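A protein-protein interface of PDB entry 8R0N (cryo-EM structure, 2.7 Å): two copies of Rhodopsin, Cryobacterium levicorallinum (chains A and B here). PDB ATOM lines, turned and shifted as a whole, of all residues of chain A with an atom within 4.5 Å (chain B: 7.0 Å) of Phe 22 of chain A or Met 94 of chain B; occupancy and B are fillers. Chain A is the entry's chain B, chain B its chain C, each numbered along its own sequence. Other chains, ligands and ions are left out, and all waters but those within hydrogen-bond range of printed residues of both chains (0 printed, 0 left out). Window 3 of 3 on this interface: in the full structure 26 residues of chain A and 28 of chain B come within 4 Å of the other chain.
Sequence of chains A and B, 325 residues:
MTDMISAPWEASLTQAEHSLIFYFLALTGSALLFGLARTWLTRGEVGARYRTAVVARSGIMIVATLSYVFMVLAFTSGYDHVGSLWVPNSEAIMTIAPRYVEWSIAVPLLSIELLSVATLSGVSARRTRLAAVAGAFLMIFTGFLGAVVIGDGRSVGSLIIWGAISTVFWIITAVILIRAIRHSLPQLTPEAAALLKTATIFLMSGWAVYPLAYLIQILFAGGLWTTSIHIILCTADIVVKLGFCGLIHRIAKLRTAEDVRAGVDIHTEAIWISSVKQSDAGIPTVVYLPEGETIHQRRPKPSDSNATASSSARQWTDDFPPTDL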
ATOM      1  N   HIS A  18       6.320  16.237  -5.591  1.00  0.00           N
ATOM      2  CA  HIS A  18       6.229  14.944  -6.251  1.00  0.00           C
ATOM      3  C   HIS A  18       7.201  14.904  -7.424  1.00  0.00           C
ATOM      4  O   HIS A  18       7.831  13.873  -7.676  1.00  0.00           O
ATOM      5  CB  HIS A  18       4.811  14.687  -6.761  1.00  0.00           C
ATOM      6  CG  HIS A  18       4.502  13.304  -7.182  1.00  0.00           C
ATOM      7  ND1 HIS A  18       4.346  12.922  -8.496  1.00  0.00           N
ATOM      8  CD2 HIS A  18       4.261  12.204  -6.430  1.00  0.00           C
ATOM      9  CE1 HIS A  18       4.073  11.606  -8.531  1.00  0.00           C
ATOM     10  NE2 HIS A  18       3.997  11.143  -7.285  1.00  0.00           N
ATOM     11  N   SER A  19       7.295  16.020  -8.149  1.00  0.00           N
ATOM     12  CA  SER A  19       8.103  16.048  -9.353  1.00  0.00           C
ATOM     13  C   SER A  19       9.578  16.007  -8.975  1.00  0.00           C
ATOM     14  O   SER A  19      10.304  15.151  -9.489  1.00  0.00           O
ATOM     15  CB  SER A  19       7.771  17.233 -10.233  1.00  0.00           C
ATOM     16  OG  SER A  19       6.557  17.006 -10.947  1.00  0.00           O
ATOM     17  N   LEU A  20       9.993  16.903  -8.065  1.00  0.00           N
ATOM     18  CA  LEU A  20      11.361  16.896  -7.578  1.00  0.00           C
ATOM     19  C   LEU A  20      11.773  15.501  -7.106  1.00  0.00           C
ATOM     20  O   LEU A  20      12.795  14.974  -7.531  1.00  0.00           O
ATOM     21  CB  LEU A  20      11.480  17.903  -6.458  1.00  0.00           C
ATOM     22  CG  LEU A  20      11.564  19.319  -6.969  1.00  0.00           C
ATOM     23  CD1 LEU A  20      11.612  20.284  -5.814  1.00  0.00           C
ATOM     24  CD2 LEU A  20      12.779  19.510  -7.871  1.00  0.00           C
ATOM     25  N   ILE A  21      10.945  14.838  -6.315  1.00  0.00           N
ATOM     26  CA  ILE A  21      11.346  13.557  -5.790  1.00  0.00           C
ATOM     27  C   ILE A  21      11.533  12.558  -6.923  1.00  0.00           C
ATOM     28  O   ILE A  21      12.425  11.725  -6.856  1.00  0.00           O
ATOM     29  CB  ILE A  21      10.362  13.063  -4.727  1.00  0.00           C
ATOM     30  CG1 ILE A  21      10.393  13.979  -3.507  1.00  0.00           C
ATOM     31  CG2 ILE A  21      10.678  11.625  -4.371  1.00  0.00           C
ATOM     32  CD1 ILE A  21       9.370  13.629  -2.444  1.00  0.00           C
ATOM     33  N   PHE A  22      10.689  12.582  -7.937  1.00  0.00           N
ATOM     34  CA  PHE A  22      10.814  11.594  -8.999  1.00  0.00           C
ATOM     35  C   PHE A  22      12.092  11.883  -9.776  1.00  0.00           C
ATOM     36  O   PHE A  22      12.780  10.964 -10.212  1.00  0.00           O
ATOM     37  CB  PHE A  22       9.616  11.613  -9.957  1.00  0.00           C
ATOM     38  CG  PHE A  22       9.917  11.115 -11.360  1.00  0.00           C
ATOM     39  CD1 PHE A  22      10.011   9.749 -11.635  1.00  0.00           C
ATOM     40  CD2 PHE A  22      10.168  12.011 -12.416  1.00  0.00           C
ATOM     41  CE1 PHE A  22      10.350   9.300 -12.918  1.00  0.00           C
ATOM     42  CE2 PHE A  22      10.504  11.554 -13.689  1.00  0.00           C
ATOM     43  CZ  PHE A  22      10.612  10.198 -13.937  1.00  0.00           C
ATOM     44  N   TYR A  23      12.392  13.168  -9.951  1.00  0.00           N
ATOM     45  CA  TYR A  23      13.578  13.542 -10.683  1.00  0.00           C
ATOM     46  C   TYR A  23      14.797  12.973  -9.975  1.00  0.00           C
ATOM     47  O   TYR A  23      15.523  12.164 -10.562  1.00  0.00           O
ATOM     48  CB  TYR A  23      13.666  15.044 -10.743  1.00  0.00           C
ATOM     49  CG  TYR A  23      14.902  15.572 -11.434  1.00  0.00           C
ATOM     50  CD1 TYR A  23      15.035  15.538 -12.810  1.00  0.00           C
ATOM     51  CD2 TYR A  23      15.900  16.182 -10.704  1.00  0.00           C
ATOM     52  CE1 TYR A  23      16.123  16.109 -13.442  1.00  0.00           C
ATOM     53  CE2 TYR A  23      17.006  16.734 -11.322  1.00  0.00           C
ATOM     54  CZ  TYR A  23      17.117  16.705 -12.694  1.00  0.00           C
ATOM     55  OH  TYR A  23      18.227  17.258 -13.252  1.00  0.00           O
ATOM     56  N   PHE A  24      14.947  13.313  -8.682  1.00  0.00           N
ATOM     57  CA  PHE A  24      16.107  12.899  -7.913  1.00  0.00           C
ATOM     58  C   PHE A  24      16.185  11.395  -7.802  1.00  0.00           C
ATOM     59  O   PHE A  24      17.255  10.830  -7.952  1.00  0.00           O
ATOM     60  CB  PHE A  24      16.146  13.598  -6.581  1.00  0.00           C
ATOM     61  CG  PHE A  24      16.659  15.000  -6.729  1.00  0.00           C
ATOM     62  CD1 PHE A  24      18.014  15.262  -6.765  1.00  0.00           C
ATOM     63  CD2 PHE A  24      15.776  16.064  -6.845  1.00  0.00           C
ATOM     64  CE1 PHE A  24      18.465  16.567  -6.871  1.00  0.00           C
ATOM     65  CE2 PHE A  24      16.225  17.366  -6.934  1.00  0.00           C
ATOM     66  CZ  PHE A  24      17.576  17.615  -6.944  1.00  0.00           C
ATOM     67  N   LEU A  25      15.083  10.737  -7.605  1.00  0.00           N
ATOM     68  CA  LEU A  25      15.179   9.308  -7.515  1.00  0.00           C
ATOM     69  C   LEU A  25      15.726   8.736  -8.799  1.00  0.00           C
ATOM     70  O   LEU A  25      16.570   7.859  -8.758  1.00  0.00           O
ATOM     71  CB  LEU A  25      13.809   8.702  -7.220  1.00  0.00           C
ATOM     72  CG  LEU A  25      13.377   8.767  -5.760  1.00  0.00           C
ATOM     73  CD1 LEU A  25      12.069   8.021  -5.635  1.00  0.00           C
ATOM     74  CD2 LEU A  25      14.411   8.163  -4.815  1.00  0.00           C
ATOM     75  N   ALA A  26      15.218   9.233  -9.925  1.00  0.00           N
ATOM     76  CA  ALA A  26      15.547   8.713 -11.239  1.00  0.00           C
ATOM     77  C   ALA A  26      16.954   9.151 -11.633  1.00  0.00           C
ATOM     78  O   ALA A  26      17.709   8.395 -12.243  1.00  0.00           O
ATOM     79  CB  ALA A  26      14.511   9.201 -12.197  1.00  0.00           C
ATOM     80  N   PHE A  75       7.460   4.618  -6.205  1.00  0.00           N
ATOM     81  CA  PHE A  75       7.060   6.003  -6.066  1.00  0.00           C
ATOM     82  C   PHE A  75       5.875   6.229  -6.986  1.00  0.00           C
ATOM     83  O   PHE A  75       4.905   6.888  -6.604  1.00  0.00           O
ATOM     84  CB  PHE A  75       8.195   6.963  -6.431  1.00  0.00           C
ATOM     85  CG  PHE A  75       7.915   8.421  -6.165  1.00  0.00           C
ATOM     86  CD1 PHE A  75       7.903   8.910  -4.871  1.00  0.00           C
ATOM     87  CD2 PHE A  75       7.666   9.298  -7.205  1.00  0.00           C
ATOM     88  CE1 PHE A  75       7.653  10.249  -4.614  1.00  0.00           C
ATOM     89  CE2 PHE A  75       7.442  10.643  -6.961  1.00  0.00           C
ATOM     90  CZ  PHE A  75       7.413  11.115  -5.657  1.00  0.00           C
ATOM     91  N   TRP B   9       1.782  17.716 -22.168  1.00  0.00           N
ATOM     92  CA  TRP B   9       1.202  16.423 -21.822  1.00  0.00           C
ATOM     93  C   TRP B   9      -0.274  16.557 -21.448  1.00  0.00           C
ATOM     94  O   TRP B   9      -0.878  15.589 -20.979  1.00  0.00           O
ATOM     95  CB  TRP B   9       1.986  15.759 -20.680  1.00  0.00           C
ATOM     96  CG  TRP B   9       2.179  16.673 -19.496  1.00  0.00           C
ATOM     97  CD1 TRP B   9       1.326  16.869 -18.452  1.00  0.00           C
ATOM     98  CD2 TRP B   9       3.288  17.569 -19.271  1.00  0.00           C
ATOM     99  NE1 TRP B   9       1.836  17.793 -17.582  1.00  0.00           N
ATOM    100  CE2 TRP B   9       3.033  18.242 -18.057  1.00  0.00           C
ATOM    101  CE3 TRP B   9       4.469  17.859 -19.968  1.00  0.00           C
ATOM    102  CZ2 TRP B   9       3.917  19.182 -17.532  1.00  0.00           C
ATOM    103  CZ3 TRP B   9       5.331  18.805 -19.458  1.00  0.00           C
ATOM    104  CH2 TRP B   9       5.052  19.462 -18.262  1.00  0.00           C
ATOM    105  N   SER B  67      15.549   5.851 -20.266  1.00  0.00           N
ATOM    106  CA  SER B  67      14.623   6.943 -20.421  1.00  0.00           C
ATOM    107  C   SER B  67      13.543   6.602 -21.448  1.00  0.00           C
ATOM    108  O   SER B  67      12.368   6.831 -21.193  1.00  0.00           O
ATOM    109  CB  SER B  67      15.371   8.194 -20.783  1.00  0.00           C
ATOM    110  OG  SER B  67      14.473   9.216 -21.208  1.00  0.00           O
ATOM    111  N   PHE B  70      11.138   3.719 -20.418  1.00  0.00           N
ATOM    112  CA  PHE B  70      10.183   4.256 -19.479  1.00  0.00           C
ATOM    113  C   PHE B  70       9.106   5.027 -20.242  1.00  0.00           C
ATOM    114  O   PHE B  70       7.913   4.805 -20.028  1.00  0.00           O
ATOM    115  CB  PHE B  70      10.929   5.084 -18.437  1.00  0.00           C
ATOM    116  CG  PHE B  70      10.087   5.653 -17.325  1.00  0.00           C
ATOM    117  CD1 PHE B  70       9.216   6.709 -17.557  1.00  0.00           C
ATOM    118  CD2 PHE B  70      10.160   5.128 -16.037  1.00  0.00           C
ATOM    119  CE1 PHE B  70       8.444   7.234 -16.523  1.00  0.00           C
ATOM    120  CE2 PHE B  70       9.381   5.650 -15.008  1.00  0.00           C
ATOM    121  CZ  PHE B  70       8.523   6.703 -15.253  1.00  0.00           C
ATOM    122  N   MET B  71       9.527   5.914 -21.141  1.00  0.00           N
ATOM    123  CA  MET B  71       8.617   6.826 -21.804  1.00  0.00           C
ATOM    124  C   MET B  71       7.684   6.050 -22.712  1.00  0.00           C
ATOM    125  O   MET B  71       6.511   6.392 -22.809  1.00  0.00           O
ATOM    126  CB  MET B  71       9.374   7.872 -22.612  1.00  0.00           C
ATOM    127  CG  MET B  71       9.816   9.023 -21.740  1.00  0.00           C
ATOM    128  SD  MET B  71      10.650  10.350 -22.629  1.00  0.00           S
ATOM    129  CE  MET B  71      11.853   9.437 -23.576  1.00  0.00           C
ATOM    130  N   VAL B  72       8.195   5.013 -23.363  1.00  0.00           N
ATOM    131  CA  VAL B  72       7.373   4.240 -24.281  1.00  0.00           C
ATOM    132  C   VAL B  72       6.301   3.525 -23.484  1.00  0.00           C
ATOM    133  O   VAL B  72       5.154   3.538 -23.886  1.00  0.00           O
ATOM    134  CB  VAL B  72       8.191   3.249 -25.120  1.00  0.00           C
ATOM    135  CG1 VAL B  72       7.327   2.129 -25.666  1.00  0.00           C
ATOM    136  CG2 VAL B  72       8.906   3.951 -26.269  1.00  0.00           C
ATOM    137  N   LEU B  73       6.673   2.944 -22.346  1.00  0.00           N
ATOM    138  CA  LEU B  73       5.715   2.300 -21.466  1.00  0.00           C
ATOM    139  C   LEU B  73       4.730   3.322 -20.902  1.00  0.00           C
ATOM    140  O   LEU B  73       3.527   3.077 -20.943  1.00  0.00           O
ATOM    141  CB  LEU B  73       6.458   1.563 -20.349  1.00  0.00           C
ATOM    142  CG  LEU B  73       7.357   0.418 -20.828  1.00  0.00           C
ATOM    143  CD1 LEU B  73       7.848  -0.419 -19.656  1.00  0.00           C
ATOM    144  CD2 LEU B  73       6.667  -0.468 -21.859  1.00  0.00           C
ATOM    145  N   ALA B  74       5.205   4.470 -20.428  1.00  0.00           N
ATOM    146  CA  ALA B  74       4.293   5.478 -19.905  1.00  0.00           C
ATOM    147  C   ALA B  74       3.385   6.029 -21.011  1.00  0.00           C
ATOM    148  O   ALA B  74       2.439   6.750 -20.720  1.00  0.00           O
ATOM    149  CB  ALA B  74       5.045   6.609 -19.217  1.00  0.00           C
ATOM    150  N   PHE B  75       3.711   5.783 -22.277  1.00  0.00           N
ATOM    151  CA  PHE B  75       2.890   6.302 -23.351  1.00  0.00           C
ATOM    152  C   PHE B  75       1.727   5.347 -23.536  1.00  0.00           C
ATOM    153  O   PHE B  75       0.589   5.791 -23.712  1.00  0.00           O
ATOM    154  CB  PHE B  75       3.671   6.430 -24.663  1.00  0.00           C
ATOM    155  CG  PHE B  75       2.938   7.114 -25.790  1.00  0.00           C
ATOM    156  CD1 PHE B  75       2.750   8.485 -25.770  1.00  0.00           C
ATOM    157  CD2 PHE B  75       2.449   6.400 -26.868  1.00  0.00           C
ATOM    158  CE1 PHE B  75       2.088   9.137 -26.804  1.00  0.00           C
ATOM    159  CE2 PHE B  75       1.806   7.043 -27.918  1.00  0.00           C
ATOM    160  CZ  PHE B  75       1.604   8.414 -27.875  1.00  0.00           C
ATOM    161  N   SER B  90      -2.933  10.958 -15.950  1.00  0.00           N
ATOM    162  CA  SER B  90      -2.027  11.709 -15.086  1.00  0.00           C
ATOM    163  C   SER B  90      -0.560  11.371 -15.399  1.00  0.00           C
ATOM    164  O   SER B  90       0.333  12.184 -15.151  1.00  0.00           O
ATOM    165  CB  SER B  90      -2.354  11.497 -13.622  1.00  0.00           C
ATOM    166  OG  SER B  90      -1.664  12.441 -12.807  1.00  0.00           O
ATOM    167  N   GLU B  91      -0.314  10.171 -15.957  1.00  0.00           N
ATOM    168  CA  GLU B  91       1.041   9.718 -16.258  1.00  0.00           C
ATOM    169  C   GLU B  91       1.420  10.023 -17.717  1.00  0.00           C
ATOM    170  O   GLU B  91       2.430   9.539 -18.273  1.00  0.00           O
ATOM    171  CB  GLU B  91       1.157   8.218 -16.008  1.00  0.00           C
ATOM    172  CG  GLU B  91       0.457   7.410 -17.076  1.00  0.00           C
ATOM    173  CD  GLU B  91       0.777   5.931 -17.020  1.00  0.00           C
ATOM    174  OE1 GLU B  91       1.411   5.444 -17.964  1.00  0.00           O
ATOM    175  OE2 GLU B  91       0.383   5.269 -16.032  1.00  0.00           O
ATOM    176  N   ALA B  92       0.652  10.899 -18.357  1.00  0.00           N
ATOM    177  CA  ALA B  92       1.087  11.502 -19.607  1.00  0.00           C
ATOM    178  C   ALA B  92       2.392  12.278 -19.401  1.00  0.00           C
ATOM    179  O   ALA B  92       3.284  12.205 -20.239  1.00  0.00           O
ATOM    180  CB  ALA B  92      -0.006  12.375 -20.171  1.00  0.00           C
ATOM    181  N   ILE B  93       2.531  12.990 -18.280  1.00  0.00           N
ATOM    182  CA  ILE B  93       3.749  13.742 -18.003  1.00  0.00           C
ATOM    183  C   ILE B  93       4.969  12.814 -17.955  1.00  0.00           C
ATOM    184  O   ILE B  93       6.094  13.240 -18.159  1.00  0.00           O
ATOM    185  CB  ILE B  93       3.612  14.518 -16.686  1.00  0.00           C
ATOM    186  CG1 ILE B  93       4.762  15.491 -16.464  1.00  0.00           C
ATOM    187  CG2 ILE B  93       3.488  13.541 -15.537  1.00  0.00           C
ATOM    188  CD1 ILE B  93       4.640  16.282 -15.194  1.00  0.00           C
ATOM    189  N   MET B  94       4.759  11.538 -17.677  1.00  0.00           N
ATOM    190  CA  MET B  94       5.841  10.576 -17.674  1.00  0.00           C
ATOM    191  C   MET B  94       6.244  10.205 -19.095  1.00  0.00           C
ATOM    192  O   MET B  94       7.018   9.264 -19.284  1.00  0.00           O
ATOM    193  CB  MET B  94       5.421   9.286 -16.956  1.00  0.00           C
ATOM    194  CG  MET B  94       5.399   9.432 -15.451  1.00  0.00           C
ATOM    195  SD  MET B  94       6.980   9.946 -14.763  1.00  0.00           S
ATOM    196  CE  MET B  94       6.618  11.658 -14.345  1.00  0.00           C
ATOM    197  N   THR B  95       5.679  10.884 -20.094  1.00  0.00           N
ATOM    198  CA  THR B  95       6.111  10.646 -21.462  1.00  0.00           C
ATOM    199  C   THR B  95       7.027  11.773 -21.918  1.00  0.00           C
ATOM    200  O   THR B  95       7.482  11.764 -23.058  1.00  0.00           O
ATOM    201  CB  THR B  95       4.926  10.494 -22.423  1.00  0.00           C
ATOM    202  OG1 THR B  95       4.234  11.750 -22.462  1.00  0.00           O
ATOM    203  CG2 THR B  95       4.005   9.359 -22.031  1.00  0.00           C
ATOM    204  N   ILE B  96       7.268  12.737 -21.034  1.00  0.00           N
ATOM    205  CA  ILE B  96       8.031  13.914 -21.391  1.00  0.00           C
ATOM    206  C   ILE B  96       9.072  14.227 -20.324  1.00  0.00           C
ATOM    207  O   ILE B  96      10.189  14.599 -20.646  1.00  0.00           O
ATOM    208  CB  ILE B  96       7.100  15.109 -21.660  1.00  0.00           C
ATOM    209  CG1 ILE B  96       6.114  14.766 -22.783  1.00  0.00           C
ATOM    210  CG2 ILE B  96       7.914  16.348 -22.003  1.00  0.00           C
ATOM    211  CD1 ILE B  96       5.257  15.930 -23.258  1.00  0.00           C
ATOM    212  N   ALA B  97       8.698  14.088 -19.063  1.00  0.00           N
ATOM    213  CA  ALA B  97       9.534  14.444 -17.930  1.00  0.00           C
ATOM    214  C   ALA B  97      10.818  13.622 -17.850  1.00  0.00           C
ATOM    215  O   ALA B  97      11.861  14.192 -17.538  1.00  0.00           O
ATOM    216  CB  ALA B  97       8.731  14.279 -16.671  1.00  0.00           C
ATOM    217  N   PRO B  98      10.821  12.303 -18.104  1.00  0.00           N
ATOM    218  CA  PRO B  98      12.052  11.524 -18.049  1.00  0.00           C
ATOM    219  C   PRO B  98      13.186  12.038 -18.926  1.00  0.00           C
ATOM    220  O   PRO B  98      14.344  11.788 -18.640  1.00  0.00           O
ATOM    221  CB  PRO B  98      11.660  10.131 -18.538  1.00  0.00           C
ATOM    222  CG  PRO B  98      10.180  10.068 -18.237  1.00  0.00           C
ATOM    223  CD  PRO B  98       9.661  11.480 -18.441  1.00  0.00           C
ATOM    224  N   ARG B  99      12.867  12.746 -19.995  1.00  0.00           N
ATOM    225  CA  ARG B  99      13.889  13.344 -20.821  1.00  0.00           C
ATOM    226  C   ARG B  99      14.855  14.169 -19.991  1.00  0.00           C
ATOM    227  O   ARG B  99      16.058  14.095 -20.222  1.00  0.00           O
ATOM    228  CB  ARG B  99      13.276  14.179 -21.938  1.00  0.00           C
ATOM    229  CG  ARG B  99      12.839  13.306 -23.104  1.00  0.00           C
ATOM    230  CD  ARG B  99      12.521  14.088 -24.364  1.00  0.00           C
ATOM    231  NE  ARG B  99      12.269  13.188 -25.483  1.00  0.00           N
ATOM    232  CZ  ARG B  99      11.058  12.927 -25.931  1.00  0.00           C
ATOM    233  NH1 ARG B  99      10.911  12.297 -27.075  1.00  0.00           N
ATOM    234  NH2 ARG B  99       9.990  13.367 -25.280  1.00  0.00           N
ATOM    235  N   VAL B 101      15.670  13.922 -16.926  1.00  0.00           N
ATOM    236  CA  VAL B 101      16.521  13.088 -16.116  1.00  0.00           C
ATOM    237  C   VAL B 101      17.682  12.656 -16.987  1.00  0.00           C
ATOM    238  O   VAL B 101      18.834  12.873 -16.616  1.00  0.00           O
ATOM    239  CB  VAL B 101      15.767  11.883 -15.532  1.00  0.00           C
ATOM    240  CG1 VAL B 101      16.690  10.895 -14.831  1.00  0.00           C
ATOM    241  CG2 VAL B 101      14.694  12.366 -14.585  1.00  0.00           C
ATOM    242  N   PHE B 144      14.348  22.023 -16.268  1.00  0.00           N
ATOM    243  CA  PHE B 144      13.362  21.145 -15.643  1.00  0.00           C
ATOM    244  C   PHE B 144      12.493  21.922 -14.663  1.00  0.00           C
ATOM    245  O   PHE B 144      11.317  21.634 -14.555  1.00  0.00           O
ATOM    246  CB  PHE B 144      14.081  20.010 -14.925  1.00  0.00           C
ATOM    247  CG  PHE B 144      13.228  19.112 -14.093  1.00  0.00           C
ATOM    248  CD1 PHE B 144      12.345  18.231 -14.680  1.00  0.00           C
ATOM    249  CD2 PHE B 144      13.338  19.119 -12.709  1.00  0.00           C
ATOM    250  CE1 PHE B 144      11.600  17.360 -13.897  1.00  0.00           C
ATOM    251  CE2 PHE B 144      12.565  18.273 -11.927  1.00  0.00           C
ATOM    252  CZ  PHE B 144      11.693  17.405 -12.523  1.00  0.00           C
ATOM    253  N   VAL B 148       8.622  21.787 -15.692  1.00  0.00           N
ATOM    254  CA  VAL B 148       7.910  20.679 -15.078  1.00  0.00           C
ATOM    255  C   VAL B 148       7.536  21.020 -13.652  1.00  0.00           C
ATOM    256  O   VAL B 148       6.485  20.560 -13.208  1.00  0.00           O
ATOM    257  CB  VAL B 148       8.720  19.381 -15.140  1.00  0.00           C
ATOM    258  CG1 VAL B 148       7.949  18.214 -14.563  1.00  0.00           C
ATOM    259  CG2 VAL B 148       9.135  19.071 -16.566  1.00  0.00           C
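Phe 70 of chain B touches Phe 22 of chain A. Phe 22 of chain A touches Met 94 of chain B (CZ to SD, 3.7 Å). Tyr 23 of chain A touches Val 101 of chain B (CD1 to CG2, 3.7 Å). CB of Tyr 23 of chain A touches CZ of Phe 144 of chain B, 3.6 Å away. Ala 26 of chain A touches Val 101 of chain B.
Of chain B, only Phe 70 (3.9 Å) and Met 94 (3.7 Å) come within 4 Å of Phe 22 of chain A. Of the printed residues of chain B, Tyr 23 of chain A touches Val 101 and Phe 144. Printed residues of chain A within 4 Å of Phe 70 of chain B: Phe 22. Ser 90 of chain B touches none of the printed residues of chain A. Glu 91 of chain B touches none of the printed residues of chain A. Met 94 of chain B touches just one residue of chain A: Phe 22 (3.7 Å). Of the printed residues of chain A, Phe 144 of chain B touches Tyr 23 (3.6 Å). The nearest residue of chain B that does not touch Phe 22 of chain A is Pro 98 of chain B (4.3 Å).
Of the 21 printed residues of chain B, 4 touch a printed residue of chain A. Hydrophobic or aromatic side chains of chain B that line the printed part of chain A: Phe 70, Met 94, Val 101 and Phe 144. Of the 10 printed residues of chain A, 3 touch a printed residue of chain B. Hydrophobic or aromatic side chains of chain A within 4 Å of the printed part of chain B: Phe 22, Tyr 23 and Ala 26. Among the printed residues, no Asp or Glu carboxylate lies within 4 Å of a Lys or Arg side-chain nitrogen of the other chain.
Position printed for both chains: 75. Of the 5 pairs that touch across the chains among the printed residues, none has its exchanged pair printed and touching as well.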
